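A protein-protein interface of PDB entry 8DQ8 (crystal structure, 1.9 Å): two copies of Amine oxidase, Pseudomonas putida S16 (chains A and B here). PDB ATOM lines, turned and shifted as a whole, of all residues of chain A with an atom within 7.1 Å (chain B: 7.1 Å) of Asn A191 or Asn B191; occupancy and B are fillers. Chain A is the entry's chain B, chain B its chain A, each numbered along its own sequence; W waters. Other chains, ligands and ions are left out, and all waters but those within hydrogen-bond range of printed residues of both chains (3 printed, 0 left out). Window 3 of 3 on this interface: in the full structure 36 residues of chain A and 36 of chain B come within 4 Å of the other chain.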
ATOM      1  N   LEU A  62      30.997 -20.347  -9.097  1.00  0.00           N
ATOM      2  CA  LEU A  62      31.776 -19.100  -9.017  1.00  0.00           C
ATOM      3  C   LEU A  62      33.257 -19.325  -9.325  1.00  0.00           C
ATOM      4  O   LEU A  62      34.012 -18.342  -9.410  1.00  0.00           O
ATOM      5  CB  LEU A  62      31.651 -18.469  -7.609  1.00  0.00           C
ATOM      6  CG  LEU A  62      30.237 -17.969  -7.337  1.00  0.00           C
ATOM      7  CD1 LEU A  62      30.015 -17.481  -5.862  1.00  0.00           C
ATOM      8  CD2 LEU A  62      29.907 -16.827  -8.319  1.00  0.00           C
ATOM      9  N   PHE A 113      34.187 -14.268  10.107  1.00  0.00           N
ATOM     10  CA  PHE A 113      34.851 -14.237   8.809  1.00  0.00           C
ATOM     11  C   PHE A 113      34.737 -12.864   8.179  1.00  0.00           C
ATOM     12  O   PHE A 113      35.719 -12.340   7.622  1.00  0.00           O
ATOM     13  CB  PHE A 113      34.229 -15.308   7.868  1.00  0.00           C
ATOM     14  CG  PHE A 113      35.235 -15.999   7.007  1.00  0.00           C
ATOM     15  CD1 PHE A 113      35.832 -15.342   5.965  1.00  0.00           C
ATOM     16  CD2 PHE A 113      35.553 -17.345   7.223  1.00  0.00           C
ATOM     17  CE1 PHE A 113      36.797 -15.985   5.179  1.00  0.00           C
ATOM     18  CE2 PHE A 113      36.462 -18.006   6.425  1.00  0.00           C
ATOM     19  CZ  PHE A 113      37.116 -17.305   5.401  1.00  0.00           C
ATOM     20  N   GLU A 114      33.547 -12.271   8.232  1.00  0.00           N
ATOM     21  CA  GLU A 114      33.397 -10.927   7.674  1.00  0.00           C
ATOM     22  C   GLU A 114      34.255  -9.914   8.419  1.00  0.00           C
ATOM     23  O   GLU A 114      34.809  -9.002   7.788  1.00  0.00           O
ATOM     24  CB  GLU A 114      31.907 -10.546   7.669  1.00  0.00           C
ATOM     25  CG  GLU A 114      31.089 -11.658   6.946  1.00  0.00           C
ATOM     26  CD  GLU A 114      30.101 -11.185   5.928  1.00  0.00           C
ATOM     27  OE1 GLU A 114      29.043 -10.692   6.404  1.00  0.00           O
ATOM     28  OE2 GLU A 114      30.288 -11.395   4.666  1.00  0.00           O
ATOM     29  N   ALA A 120      38.441  -6.647   2.389  1.00  0.00           N
ATOM     30  CA  ALA A 120      38.766  -7.407   1.176  1.00  0.00           C
ATOM     31  C   ALA A 120      38.480  -6.606  -0.074  1.00  0.00           C
ATOM     32  O   ALA A 120      39.203  -6.726  -1.073  1.00  0.00           O
ATOM     33  CB  ALA A 120      37.987  -8.729   1.143  1.00  0.00           C
ATOM     34  N   TRP A 121      37.420  -5.785  -0.061  1.00  0.00           N
ATOM     35  CA  TRP A 121      37.078  -4.986  -1.252  1.00  0.00           C
ATOM     36  C   TRP A 121      38.160  -3.975  -1.579  1.00  0.00           C
ATOM     37  O   TRP A 121      38.440  -3.707  -2.758  1.00  0.00           O
ATOM     38  CB  TRP A 121      35.755  -4.233  -1.016  1.00  0.00           C
ATOM     39  CG  TRP A 121      34.614  -4.835  -1.699  1.00  0.00           C
ATOM     40  CD1 TRP A 121      33.535  -5.459  -1.104  1.00  0.00           C
ATOM     41  CD2 TRP A 121      34.390  -4.906  -3.123  1.00  0.00           C
ATOM     42  NE1 TRP A 121      32.667  -5.922  -2.085  1.00  0.00           N
ATOM     43  CE2 TRP A 121      33.157  -5.564  -3.323  1.00  0.00           C
ATOM     44  CE3 TRP A 121      35.130  -4.481  -4.245  1.00  0.00           C
ATOM     45  CZ2 TRP A 121      32.646  -5.813  -4.591  1.00  0.00           C
ATOM     46  CZ3 TRP A 121      34.627  -4.707  -5.503  1.00  0.00           C
ATOM     47  CH2 TRP A 121      33.383  -5.388  -5.670  1.00  0.00           C
ATOM     48  N   PHE A 185      38.654 -14.926  -0.274  1.00  0.00           N
ATOM     49  CA  PHE A 185      37.349 -14.354   0.077  1.00  0.00           C
ATOM     50  C   PHE A 185      36.848 -13.424  -1.032  1.00  0.00           C
ATOM     51  O   PHE A 185      35.676 -13.473  -1.436  1.00  0.00           O
ATOM     52  CB  PHE A 185      37.521 -13.636   1.424  1.00  0.00           C
ATOM     53  CG  PHE A 185      36.254 -12.962   1.961  1.00  0.00           C
ATOM     54  CD1 PHE A 185      35.367 -13.664   2.767  1.00  0.00           C
ATOM     55  CD2 PHE A 185      36.000 -11.622   1.688  1.00  0.00           C
ATOM     56  CE1 PHE A 185      34.238 -13.047   3.295  1.00  0.00           C
ATOM     57  CE2 PHE A 185      34.877 -10.980   2.224  1.00  0.00           C
ATOM     58  CZ  PHE A 185      34.007 -11.665   3.033  1.00  0.00           C
ATOM     59  N   ALA A 186      37.730 -12.581  -1.557  1.00  0.00           N
ATOM     60  CA  ALA A 186      37.370 -11.750  -2.717  1.00  0.00           C
ATOM     61  C   ALA A 186      36.975 -12.599  -3.935  1.00  0.00           C
ATOM     62  O   ALA A 186      36.015 -12.272  -4.647  1.00  0.00           O
ATOM     63  CB  ALA A 186      38.558 -10.807  -3.036  1.00  0.00           C
ATOM     64  N   GLY A 188      35.480 -15.381  -3.921  1.00  0.00           N
ATOM     65  CA  GLY A 188      34.154 -15.883  -3.630  1.00  0.00           C
ATOM     66  C   GLY A 188      33.125 -14.754  -3.494  1.00  0.00           C
ATOM     67  O   GLY A 188      32.198 -14.854  -2.695  1.00  0.00           O
ATOM     68  N   GLY A 189      33.282 -13.683  -4.266  1.00  0.00           N
ATOM     69  CA  GLY A 189      32.302 -12.594  -4.309  1.00  0.00           C
ATOM     70  C   GLY A 189      32.336 -11.656  -3.105  1.00  0.00           C
ATOM     71  O   GLY A 189      31.324 -11.012  -2.826  1.00  0.00           O
ATOM     72  N   TRP A 190      33.464 -11.572  -2.398  1.00  0.00           N
ATOM     73  CA  TRP A 190      33.622 -10.665  -1.255  1.00  0.00           C
ATOM     74  C   TRP A 190      32.501 -10.808  -0.223  1.00  0.00           C
ATOM     75  O   TRP A 190      32.037  -9.833   0.370  1.00  0.00           O
ATOM     76  CB  TRP A 190      33.673  -9.196  -1.732  1.00  0.00           C
ATOM     77  CG  TRP A 190      34.742  -8.801  -2.739  1.00  0.00           C
ATOM     78  CD1 TRP A 190      36.026  -8.391  -2.470  1.00  0.00           C
ATOM     79  CD2 TRP A 190      34.568  -8.683  -4.165  1.00  0.00           C
ATOM     80  NE1 TRP A 190      36.673  -8.073  -3.673  1.00  0.00           N
ATOM     81  CE2 TRP A 190      35.797  -8.234  -4.707  1.00  0.00           C
ATOM     82  CE3 TRP A 190      33.486  -8.917  -5.028  1.00  0.00           C
ATOM     83  CZ2 TRP A 190      35.978  -7.996  -6.066  1.00  0.00           C
ATOM     84  CZ3 TRP A 190      33.661  -8.660  -6.418  1.00  0.00           C
ATOM     85  CH2 TRP A 190      34.886  -8.198  -6.912  1.00  0.00           C
ATOM     86  N   ASN A 191      32.028 -12.018   0.011  1.00  0.00           N
ATOM     87  CA  ASN A 191      31.000 -12.174   1.018  1.00  0.00           C
ATOM     88  C   ASN A 191      31.021 -13.609   1.530  1.00  0.00           C
ATOM     89  O   ASN A 191      31.356 -14.564   0.815  1.00  0.00           O
ATOM     90  CB  ASN A 191      29.649 -11.678   0.456  1.00  0.00           C
ATOM     91  CG  ASN A 191      28.861 -12.735  -0.295  1.00  0.00           C
ATOM     92  OD1 ASN A 191      28.142 -13.579   0.288  1.00  0.00           O
ATOM     93  ND2 ASN A 191      28.990 -12.693  -1.597  1.00  0.00           N
ATOM     94  N   TYR A 192      30.764 -13.729   2.839  1.00  0.00           N
ATOM     95  CA  TYR A 192      30.973 -15.004   3.516  1.00  0.00           C
ATOM     96  C   TYR A 192      30.027 -16.089   3.000  1.00  0.00           C
ATOM     97  O   TYR A 192      30.453 -17.245   2.790  1.00  0.00           O
ATOM     98  CB  TYR A 192      30.817 -14.864   5.045  1.00  0.00           C
ATOM     99  CG  TYR A 192      30.846 -16.258   5.682  1.00  0.00           C
ATOM    100  CD1 TYR A 192      32.047 -16.984   5.788  1.00  0.00           C
ATOM    101  CD2 TYR A 192      29.666 -16.883   6.092  1.00  0.00           C
ATOM    102  CE1 TYR A 192      32.062 -18.297   6.356  1.00  0.00           C
ATOM    103  CE2 TYR A 192      29.668 -18.165   6.626  1.00  0.00           C
ATOM    104  CZ  TYR A 192      30.870 -18.868   6.758  1.00  0.00           C
ATOM    105  OH  TYR A 192      30.853 -20.180   7.291  1.00  0.00           O
ATOM    106  N   ASP A 193      28.715 -15.783   2.878  1.00  0.00           N
ATOM    107  CA  ASP A 193      27.766 -16.829   2.466  1.00  0.00           C
ATOM    108  C   ASP A 193      28.162 -17.451   1.106  1.00  0.00           C
ATOM    109  O   ASP A 193      28.214 -18.700   0.948  1.00  0.00           O
ATOM    110  CB  ASP A 193      26.356 -16.274   2.398  1.00  0.00           C
ATOM    111  CG  ASP A 193      25.771 -15.965   3.788  1.00  0.00           C
ATOM    112  OD1 ASP A 193      26.157 -16.613   4.752  1.00  0.00           O
ATOM    113  OD2 ASP A 193      24.865 -15.136   3.885  1.00  0.00           O
ATOM    114  N   ALA A 194      28.483 -16.597   0.120  1.00  0.00           N
ATOM    115  CA  ALA A 194      28.947 -17.104  -1.182  1.00  0.00           C
ATOM    116  C   ALA A 194      30.252 -17.898  -1.039  1.00  0.00           C
ATOM    117  O   ALA A 194      30.382 -19.042  -1.544  1.00  0.00           O
ATOM    118  CB  ALA A 194      29.139 -15.927  -2.161  1.00  0.00           C
ATOM    119  N   PHE A 195      31.242 -17.307  -0.340  1.00  0.00           N
ATOM    120  CA  PHE A 195      32.541 -17.979  -0.217  1.00  0.00           C
ATOM    121  C   PHE A 195      32.405 -19.344   0.445  1.00  0.00           C
ATOM    122  O   PHE A 195      32.940 -20.346  -0.060  1.00  0.00           O
ATOM    123  CB  PHE A 195      33.537 -17.127   0.580  1.00  0.00           C
ATOM    124  CG  PHE A 195      34.829 -17.843   0.833  1.00  0.00           C
ATOM    125  CD1 PHE A 195      35.773 -17.951  -0.169  1.00  0.00           C
ATOM    126  CD2 PHE A 195      35.058 -18.463   2.062  1.00  0.00           C
ATOM    127  CE1 PHE A 195      36.964 -18.659   0.032  1.00  0.00           C
ATOM    128  CE2 PHE A 195      36.233 -19.171   2.270  1.00  0.00           C
ATOM    129  CZ  PHE A 195      37.188 -19.260   1.283  1.00  0.00           C
ATOM    130  N   MET A 196      31.701 -19.414   1.573  1.00  0.00           N
ATOM    131  CA  MET A 196      31.475 -20.728   2.214  1.00  0.00           C
ATOM    132  C   MET A 196      30.809 -21.721   1.259  1.00  0.00           C
ATOM    133  O   MET A 196      31.154 -22.927   1.229  1.00  0.00           O
ATOM    134  CB  MET A 196      30.639 -20.535   3.474  1.00  0.00           C
ATOM    135  CG  MET A 196      30.583 -21.755   4.441  1.00  0.00           C
ATOM    136  SD  MET A 196      32.023 -22.791   4.653  1.00  0.00           S
ATOM    137  CE  MET A 196      31.570 -23.632   6.150  1.00  0.00           C
ATOM    138  N   ASP A 197      29.812 -21.265   0.496  1.00  0.00           N
ATOM    139  CA  ASP A 197      29.171 -22.203  -0.436  1.00  0.00           C
ATOM    140  C   ASP A 197      30.170 -22.787  -1.442  1.00  0.00           C
ATOM    141  O   ASP A 197      29.977 -23.928  -1.938  1.00  0.00           O
ATOM    142  CB  ASP A 197      28.057 -21.469  -1.178  1.00  0.00           C
ATOM    143  CG  ASP A 197      26.958 -22.423  -1.684  1.00  0.00           C
ATOM    144  OD1 ASP A 197      26.525 -23.273  -0.890  1.00  0.00           O
ATOM    145  OD2 ASP A 197      26.536 -22.297  -2.866  1.00  0.00           O
ATOM    146  N   LEU B  62      33.829 -13.255 -12.153  1.00  0.00           N
ATOM    147  CA  LEU B  62      32.782 -14.110 -11.587  1.00  0.00           C
ATOM    148  C   LEU B  62      31.944 -14.757 -12.692  1.00  0.00           C
ATOM    149  O   LEU B  62      31.085 -15.607 -12.390  1.00  0.00           O
ATOM    150  CB  LEU B  62      31.841 -13.299 -10.664  1.00  0.00           C
ATOM    151  CG  LEU B  62      32.536 -12.797  -9.397  1.00  0.00           C
ATOM    152  CD1 LEU B  62      31.647 -11.887  -8.522  1.00  0.00           C
ATOM    153  CD2 LEU B  62      32.971 -14.021  -8.545  1.00  0.00           C
ATOM    154  N   PHE B 113      18.290  -2.743  -4.181  1.00  0.00           N
ATOM    155  CA  PHE B 113      18.538  -3.999  -4.885  1.00  0.00           C
ATOM    156  C   PHE B 113      18.504  -5.168  -3.923  1.00  0.00           C
ATOM    157  O   PHE B 113      17.941  -6.226  -4.249  1.00  0.00           O
ATOM    158  CB  PHE B 113      19.908  -3.936  -5.627  1.00  0.00           C
ATOM    159  CG  PHE B 113      19.904  -4.613  -6.967  1.00  0.00           C
ATOM    160  CD1 PHE B 113      19.839  -5.971  -7.053  1.00  0.00           C
ATOM    161  CD2 PHE B 113      20.060  -3.882  -8.138  1.00  0.00           C
ATOM    162  CE1 PHE B 113      19.829  -6.615  -8.294  1.00  0.00           C
ATOM    163  CE2 PHE B 113      20.091  -4.501  -9.368  1.00  0.00           C
ATOM    164  CZ  PHE B 113      19.949  -5.876  -9.453  1.00  0.00           C
ATOM    165  N   GLU B 114      19.124  -5.008  -2.745  1.00  0.00           N
ATOM    166  CA  GLU B 114      19.111  -6.101  -1.770  1.00  0.00           C
ATOM    167  C   GLU B 114      17.689  -6.391  -1.302  1.00  0.00           C
ATOM    168  O   GLU B 114      17.327  -7.559  -1.074  1.00  0.00           O
ATOM    169  CB  GLU B 114      20.044  -5.766  -0.592  1.00  0.00           C
ATOM    170  CG  GLU B 114      21.533  -5.670  -1.046  1.00  0.00           C
ATOM    171  CD  GLU B 114      22.327  -6.988  -0.945  1.00  0.00           C
ATOM    172  OE1 GLU B 114      23.564  -6.994  -1.155  1.00  0.00           O
ATOM    173  OE2 GLU B 114      21.692  -8.072  -0.602  1.00  0.00           O
ATOM    174  N   ALA B 120      16.909 -14.260  -2.820  1.00  0.00           N
ATOM    175  CA  ALA B 120      17.638 -14.918  -3.913  1.00  0.00           C
ATOM    176  C   ALA B 120      18.301 -16.198  -3.458  1.00  0.00           C
ATOM    177  O   ALA B 120      18.397 -17.142  -4.237  1.00  0.00           O
ATOM    178  CB  ALA B 120      18.685 -13.979  -4.512  1.00  0.00           C
ATOM    179  N   TRP B 121      18.778 -16.253  -2.205  1.00  0.00           N
ATOM    180  CA  TRP B 121      19.433 -17.469  -1.706  1.00  0.00           C
ATOM    181  C   TRP B 121      18.463 -18.633  -1.634  1.00  0.00           C
ATOM    182  O   TRP B 121      18.841 -19.775  -1.919  1.00  0.00           O
ATOM    183  CB  TRP B 121      20.007 -17.232  -0.298  1.00  0.00           C
ATOM    184  CG  TRP B 121      21.441 -17.064  -0.293  1.00  0.00           C
ATOM    185  CD1 TRP B 121      22.126 -15.881  -0.027  1.00  0.00           C
ATOM    186  CD2 TRP B 121      22.442 -18.060  -0.577  1.00  0.00           C
ATOM    187  NE1 TRP B 121      23.492 -16.109  -0.148  1.00  0.00           N
ATOM    188  CE2 TRP B 121      23.710 -17.439  -0.439  1.00  0.00           C
ATOM    189  CE3 TRP B 121      22.385 -19.425  -0.927  1.00  0.00           C
ATOM    190  CZ2 TRP B 121      24.905 -18.136  -0.639  1.00  0.00           C
ATOM    191  CZ3 TRP B 121      23.552 -20.115  -1.119  1.00  0.00           C
ATOM    192  CH2 TRP B 121      24.814 -19.463  -0.993  1.00  0.00           C
ATOM    193  N   PHE B 185      21.169 -11.987 -10.024  1.00  0.00           N
ATOM    194  CA  PHE B 185      21.734 -11.576  -8.732  1.00  0.00           C
ATOM    195  C   PHE B 185      22.432 -12.748  -8.036  1.00  0.00           C
ATOM    196  O   PHE B 185      23.544 -12.611  -7.487  1.00  0.00           O
ATOM    197  CB  PHE B 185      20.588 -10.990  -7.902  1.00  0.00           C
ATOM    198  CG  PHE B 185      20.997 -10.480  -6.525  1.00  0.00           C
ATOM    199  CD1 PHE B 185      21.466  -9.164  -6.361  1.00  0.00           C
ATOM    200  CD2 PHE B 185      20.880 -11.296  -5.416  1.00  0.00           C
ATOM    201  CE1 PHE B 185      21.803  -8.672  -5.119  1.00  0.00           C
ATOM    202  CE2 PHE B 185      21.231 -10.808  -4.133  1.00  0.00           C
ATOM    203  CZ  PHE B 185      21.660  -9.515  -3.975  1.00  0.00           C
ATOM    204  N   ALA B 186      21.797 -13.928  -8.051  1.00  0.00           N
ATOM    205  CA  ALA B 186      22.429 -15.143  -7.518  1.00  0.00           C
ATOM    206  C   ALA B 186      23.725 -15.476  -8.267  1.00  0.00           C
ATOM    207  O   ALA B 186      24.739 -15.821  -7.651  1.00  0.00           O
ATOM    208  CB  ALA B 186      21.428 -16.344  -7.634  1.00  0.00           C
ATOM    209  N   GLY B 188      25.784 -13.454  -9.507  1.00  0.00           N
ATOM    210  CA  GLY B 188      26.770 -12.511  -9.030  1.00  0.00           C
ATOM    211  C   GLY B 188      27.081 -12.638  -7.543  1.00  0.00           C
ATOM    212  O   GLY B 188      27.346 -11.638  -6.890  1.00  0.00           O
ATOM    213  N   GLY B 189      27.050 -13.851  -7.000  1.00  0.00           N
ATOM    214  CA  GLY B 189      27.410 -14.090  -5.603  1.00  0.00           C
ATOM    215  C   GLY B 189      26.355 -13.668  -4.581  1.00  0.00           C
ATOM    216  O   GLY B 189      26.714 -13.442  -3.421  1.00  0.00           O
ATOM    217  N   TRP B 190      25.078 -13.577  -4.978  1.00  0.00           N
ATOM    218  CA  TRP B 190      23.975 -13.251  -4.067  1.00  0.00           C
ATOM    219  C   TRP B 190      24.236 -11.978  -3.260  1.00  0.00           C
ATOM    220  O   TRP B 190      23.856 -11.867  -2.085  1.00  0.00           O
ATOM    221  CB  TRP B 190      23.715 -14.422  -3.094  1.00  0.00           C
ATOM    222  CG  TRP B 190      23.363 -15.770  -3.678  1.00  0.00           C
ATOM    223  CD1 TRP B 190      22.133 -16.216  -4.064  1.00  0.00           C
ATOM    224  CD2 TRP B 190      24.271 -16.869  -3.878  1.00  0.00           C
ATOM    225  NE1 TRP B 190      22.213 -17.541  -4.499  1.00  0.00           N
ATOM    226  CE2 TRP B 190      23.514 -17.954  -4.388  1.00  0.00           C
ATOM    227  CE3 TRP B 190      25.642 -17.045  -3.632  1.00  0.00           C
ATOM    228  CZ2 TRP B 190      24.070 -19.190  -4.654  1.00  0.00           C
ATOM    229  CZ3 TRP B 190      26.223 -18.306  -3.910  1.00  0.00           C
ATOM    230  CH2 TRP B 190      25.425 -19.364  -4.402  1.00  0.00           C
ATOM    231  N   ASN B 191      24.866 -10.983  -3.874  1.00  0.00           N
ATOM    232  CA  ASN B 191      25.122  -9.753  -3.142  1.00  0.00           C
ATOM    233  C   ASN B 191      25.328  -8.602  -4.126  1.00  0.00           C
ATOM    234  O   ASN B 191      25.865  -8.766  -5.232  1.00  0.00           O
ATOM    235  CB  ASN B 191      26.271  -9.972  -2.131  1.00  0.00           C
ATOM    236  CG  ASN B 191      27.650  -9.693  -2.689  1.00  0.00           C
ATOM    237  OD1 ASN B 191      28.332 -10.651  -3.091  1.00  0.00           O
ATOM    238  ND2 ASN B 191      28.112  -8.427  -2.631  1.00  0.00           N
ATOM    239  N   TYR B 192      24.808  -7.435  -3.731  1.00  0.00           N
ATOM    240  CA  TYR B 192      24.722  -6.314  -4.659  1.00  0.00           C
ATOM    241  C   TYR B 192      26.101  -5.804  -5.078  1.00  0.00           C
ATOM    242  O   TYR B 192      26.321  -5.503  -6.265  1.00  0.00           O
ATOM    243  CB  TYR B 192      23.909  -5.141  -4.057  1.00  0.00           C
ATOM    244  CG  TYR B 192      23.984  -3.934  -5.000  1.00  0.00           C
ATOM    245  CD1 TYR B 192      23.251  -3.887  -6.205  1.00  0.00           C
ATOM    246  CD2 TYR B 192      24.853  -2.871  -4.720  1.00  0.00           C
ATOM    247  CE1 TYR B 192      23.367  -2.763  -7.093  1.00  0.00           C
ATOM    248  CE2 TYR B 192      24.998  -1.787  -5.586  1.00  0.00           C
ATOM    249  CZ  TYR B 192      24.252  -1.740  -6.771  1.00  0.00           C
ATOM    250  OH  TYR B 192      24.400  -0.622  -7.626  1.00  0.00           O
ATOM    251  N   ASP B 193      27.018  -5.590  -4.113  1.00  0.00           N
ATOM    252  CA  ASP B 193      28.320  -5.019  -4.489  1.00  0.00           C
ATOM    253  C   ASP B 193      29.025  -5.889  -5.551  1.00  0.00           C
ATOM    254  O   ASP B 193      29.532  -5.385  -6.581  1.00  0.00           O
ATOM    255  CB  ASP B 193      29.196  -4.834  -3.271  1.00  0.00           C
ATOM    256  CG  ASP B 193      28.639  -3.772  -2.288  1.00  0.00           C
ATOM    257  OD1 ASP B 193      28.091  -2.787  -2.746  1.00  0.00           O
ATOM    258  OD2 ASP B 193      28.817  -3.899  -1.076  1.00  0.00           O
ATOM    259  N   ALA B 194      29.043  -7.216  -5.331  1.00  0.00           N
ATOM    260  CA  ALA B 194      29.640  -8.120  -6.328  1.00  0.00           C
ATOM    261  C   ALA B 194      28.895  -8.053  -7.658  1.00  0.00           C
ATOM    262  O   ALA B 194      29.507  -7.902  -8.749  1.00  0.00           O
ATOM    263  CB  ALA B 194      29.652  -9.562  -5.769  1.00  0.00           C
ATOM    264  N   PHE B 195      27.557  -8.165  -7.606  1.00  0.00           N
ATOM    265  CA  PHE B 195      26.774  -8.176  -8.850  1.00  0.00           C
ATOM    266  C   PHE B 195      26.976  -6.902  -9.657  1.00  0.00           C
ATOM    267  O   PHE B 195      27.218  -6.947 -10.862  1.00  0.00           O
ATOM    268  CB  PHE B 195      25.280  -8.353  -8.570  1.00  0.00           C
ATOM    269  CG  PHE B 195      24.436  -8.253  -9.809  1.00  0.00           C
ATOM    270  CD1 PHE B 195      24.345  -9.322 -10.680  1.00  0.00           C
ATOM    271  CD2 PHE B 195      23.774  -7.075 -10.122  1.00  0.00           C
ATOM    272  CE1 PHE B 195      23.590  -9.240 -11.837  1.00  0.00           C
ATOM    273  CE2 PHE B 195      23.033  -6.964 -11.285  1.00  0.00           C
ATOM    274  CZ  PHE B 195      22.920  -8.038 -12.144  1.00  0.00           C
ATOM    275  N   MET B 196      26.868  -5.747  -9.012  1.00  0.00           N
ATOM    276  CA  MET B 196      27.117  -4.485  -9.717  1.00  0.00           C
ATOM    277  C   MET B 196      28.494  -4.451 -10.350  1.00  0.00           C
ATOM    278  O   MET B 196      28.654  -3.963 -11.485  1.00  0.00           O
ATOM    279  CB  MET B 196      26.890  -3.327  -8.764  1.00  0.00           C
ATOM    280  CG  MET B 196      26.880  -1.923  -9.406  1.00  0.00           C
ATOM    281  SD  MET B 196      26.007  -1.688 -10.928  1.00  0.00           S
ATOM    282  CE  MET B 196      25.841   0.082 -10.951  1.00  0.00           C
ATOM    283  N   ASP B 197      29.523  -4.928  -9.627  1.00  0.00           N
ATOM    284  CA  ASP B 197      30.860  -4.905 -10.224  1.00  0.00           C
ATOM    285  C   ASP B 197      30.913  -5.738 -11.520  1.00  0.00           C
ATOM    286  O   ASP B 197      31.718  -5.440 -12.428  1.00  0.00           O
ATOM    287  CB  ASP B 197      31.858  -5.449  -9.205  1.00  0.00           C
ATOM    288  CG  ASP B 197      33.287  -4.989  -9.467  1.00  0.00           C
ATOM    289  OD1 ASP B 197      33.481  -3.779  -9.651  1.00  0.00           O
ATOM    290  OD2 ASP B 197      34.215  -5.862  -9.463  1.00  0.00           O
HETATM  291  O   HOH W   1      25.252 -13.579  -0.067  1.00  0.00           O
HETATM  292  O   HOH W   2      33.042 -17.748 -11.953  1.00  0.00           O
HETATM  293  O   HOH W   3      30.499  -7.925  -1.059  1.00  0.00           O
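Water W2 bridges the backbone carbonyl oxygen of Leu A62 and the backbone carbonyl oxygen of Leu B62.
Water W3 lies within hydrogen-bond range of the backbone carbonyl oxygen (O) of Trp A190 (2.8 Å), the side-chain amide nitrogen (ND2) of Asn B191 (2.9 Å) and the indole nitrogen (NE1) of Trp A121 (3.1 Å).
Water W1 lies within hydrogen-bond range of OD1 of Asn A191 (2.9 Å), O of Trp B190 (3.0 Å) and NE1 of Trp B121 (3.1 Å).
OD1 of Asn B191 lies within hydrogen-bond range of ND2 of Asn A191.
The side-chain amide oxygen of Asn B191 lies close to the backbone carbonyl oxygen of Gly A189.
The backbone carbonyl oxygen (O) of Gly B189 is in hydrogen-bond range of the side-chain amide nitrogen (ND2) of Asn A191 (3.0 Å).
Of the 17 printed residues of chain B, 7 touch a printed residue of chain A.
Printed residues of chain A that touch a printed residue of chain B: Trp A121, Gly A189, Trp A190, Asn A191, Asp A193, Ala A194 and Asp A197.
Among the printed residues, 15 pairs touch across the chains.
Trp A121 touches Ala B194, and with the chains exchanged Ala A194 touches Trp B121.
Gly A189 touches Asn B191, and with the chains exchanged Asn A191 touches Gly B189.
Trp A190 touches Ala B194, and with the chains exchanged Ala A194 touches Trp B190.
Asn A191 touches its own counterpart, Asn B191.
17 positions are printed for both chains.
Of the 15 pairs that touch across the chains among the printed residues, 15 have their exchanged pair printed and touching as well.
Of the printed residues of chain B, Asn A191 touches Gly B189 (3.0 Å) and Asn B191 (2.6 Å).
Of the printed residues of chain A, Asn B191 touches Gly A189 (3.0 Å) and Asn A191 (2.6 Å).
Of the printed residues of chain B, Trp A121 touches Asp B193, Ala B194 and Asp B197.
Of the printed residues of chain A, Asp B193 touches Trp A121.
The nearest printed residue of chain B that does not touch Asn A191 is Trp B190 (5.1 Å).
The nearest printed residue of chain A that does not touch Asn B191 is Trp A190 (5.1 Å).
The nearest printed residue of chain B that does not touch Asp A197 is Ala B186 (8.3 Å).
Among the printed residues, merely in contact across the chains: Trp A121 with Asp B193 (3.7 Å), Trp A121 with Ala B194 (3.9 Å), Trp A121 with Asp B197 (3.8 Å), Gly A189 with Ala B194 (3.7 Å), Trp A190 with Ala B194 (3.96 Å), Trp A190 with Asp B197 (3.5 Å), Asp A193 with Trp B121 (3.7 Å), Ala A194 with Trp B121 (3.97 Å), Ala A194 with Gly B189 (3.7 Å), Ala A194 with Trp B190 (3.96 Å), Asp A197 with Trp B121 (3.7 Å) and Asp A197 with Trp B190 (3.5 Å).
The side-chain amide oxygen of Asn A191 sits at hydrogen-bond distance from the backbone NH of Ala A194 (3.0 Å).
O of Phe A185 lies within hydrogen-bond range of N of Trp A190 (3.1 Å).
ND2 of Asn B191 lies close to N of Ala B194, 3.1 Å away.
The backbone carbonyl oxygen (O) of Gly B189 sits close to the side-chain amide oxygen (OD1) of Asn B191, 3.2 Å away.
The side-chain amide nitrogen (ND2) of Asn B191 lies close to the backbone NH (N) of Asp B193, at 3.4 Å.
The backbone carbonyl oxygen of Phe B185 sits at hydrogen-bond distance from the backbone NH of Trp B190.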
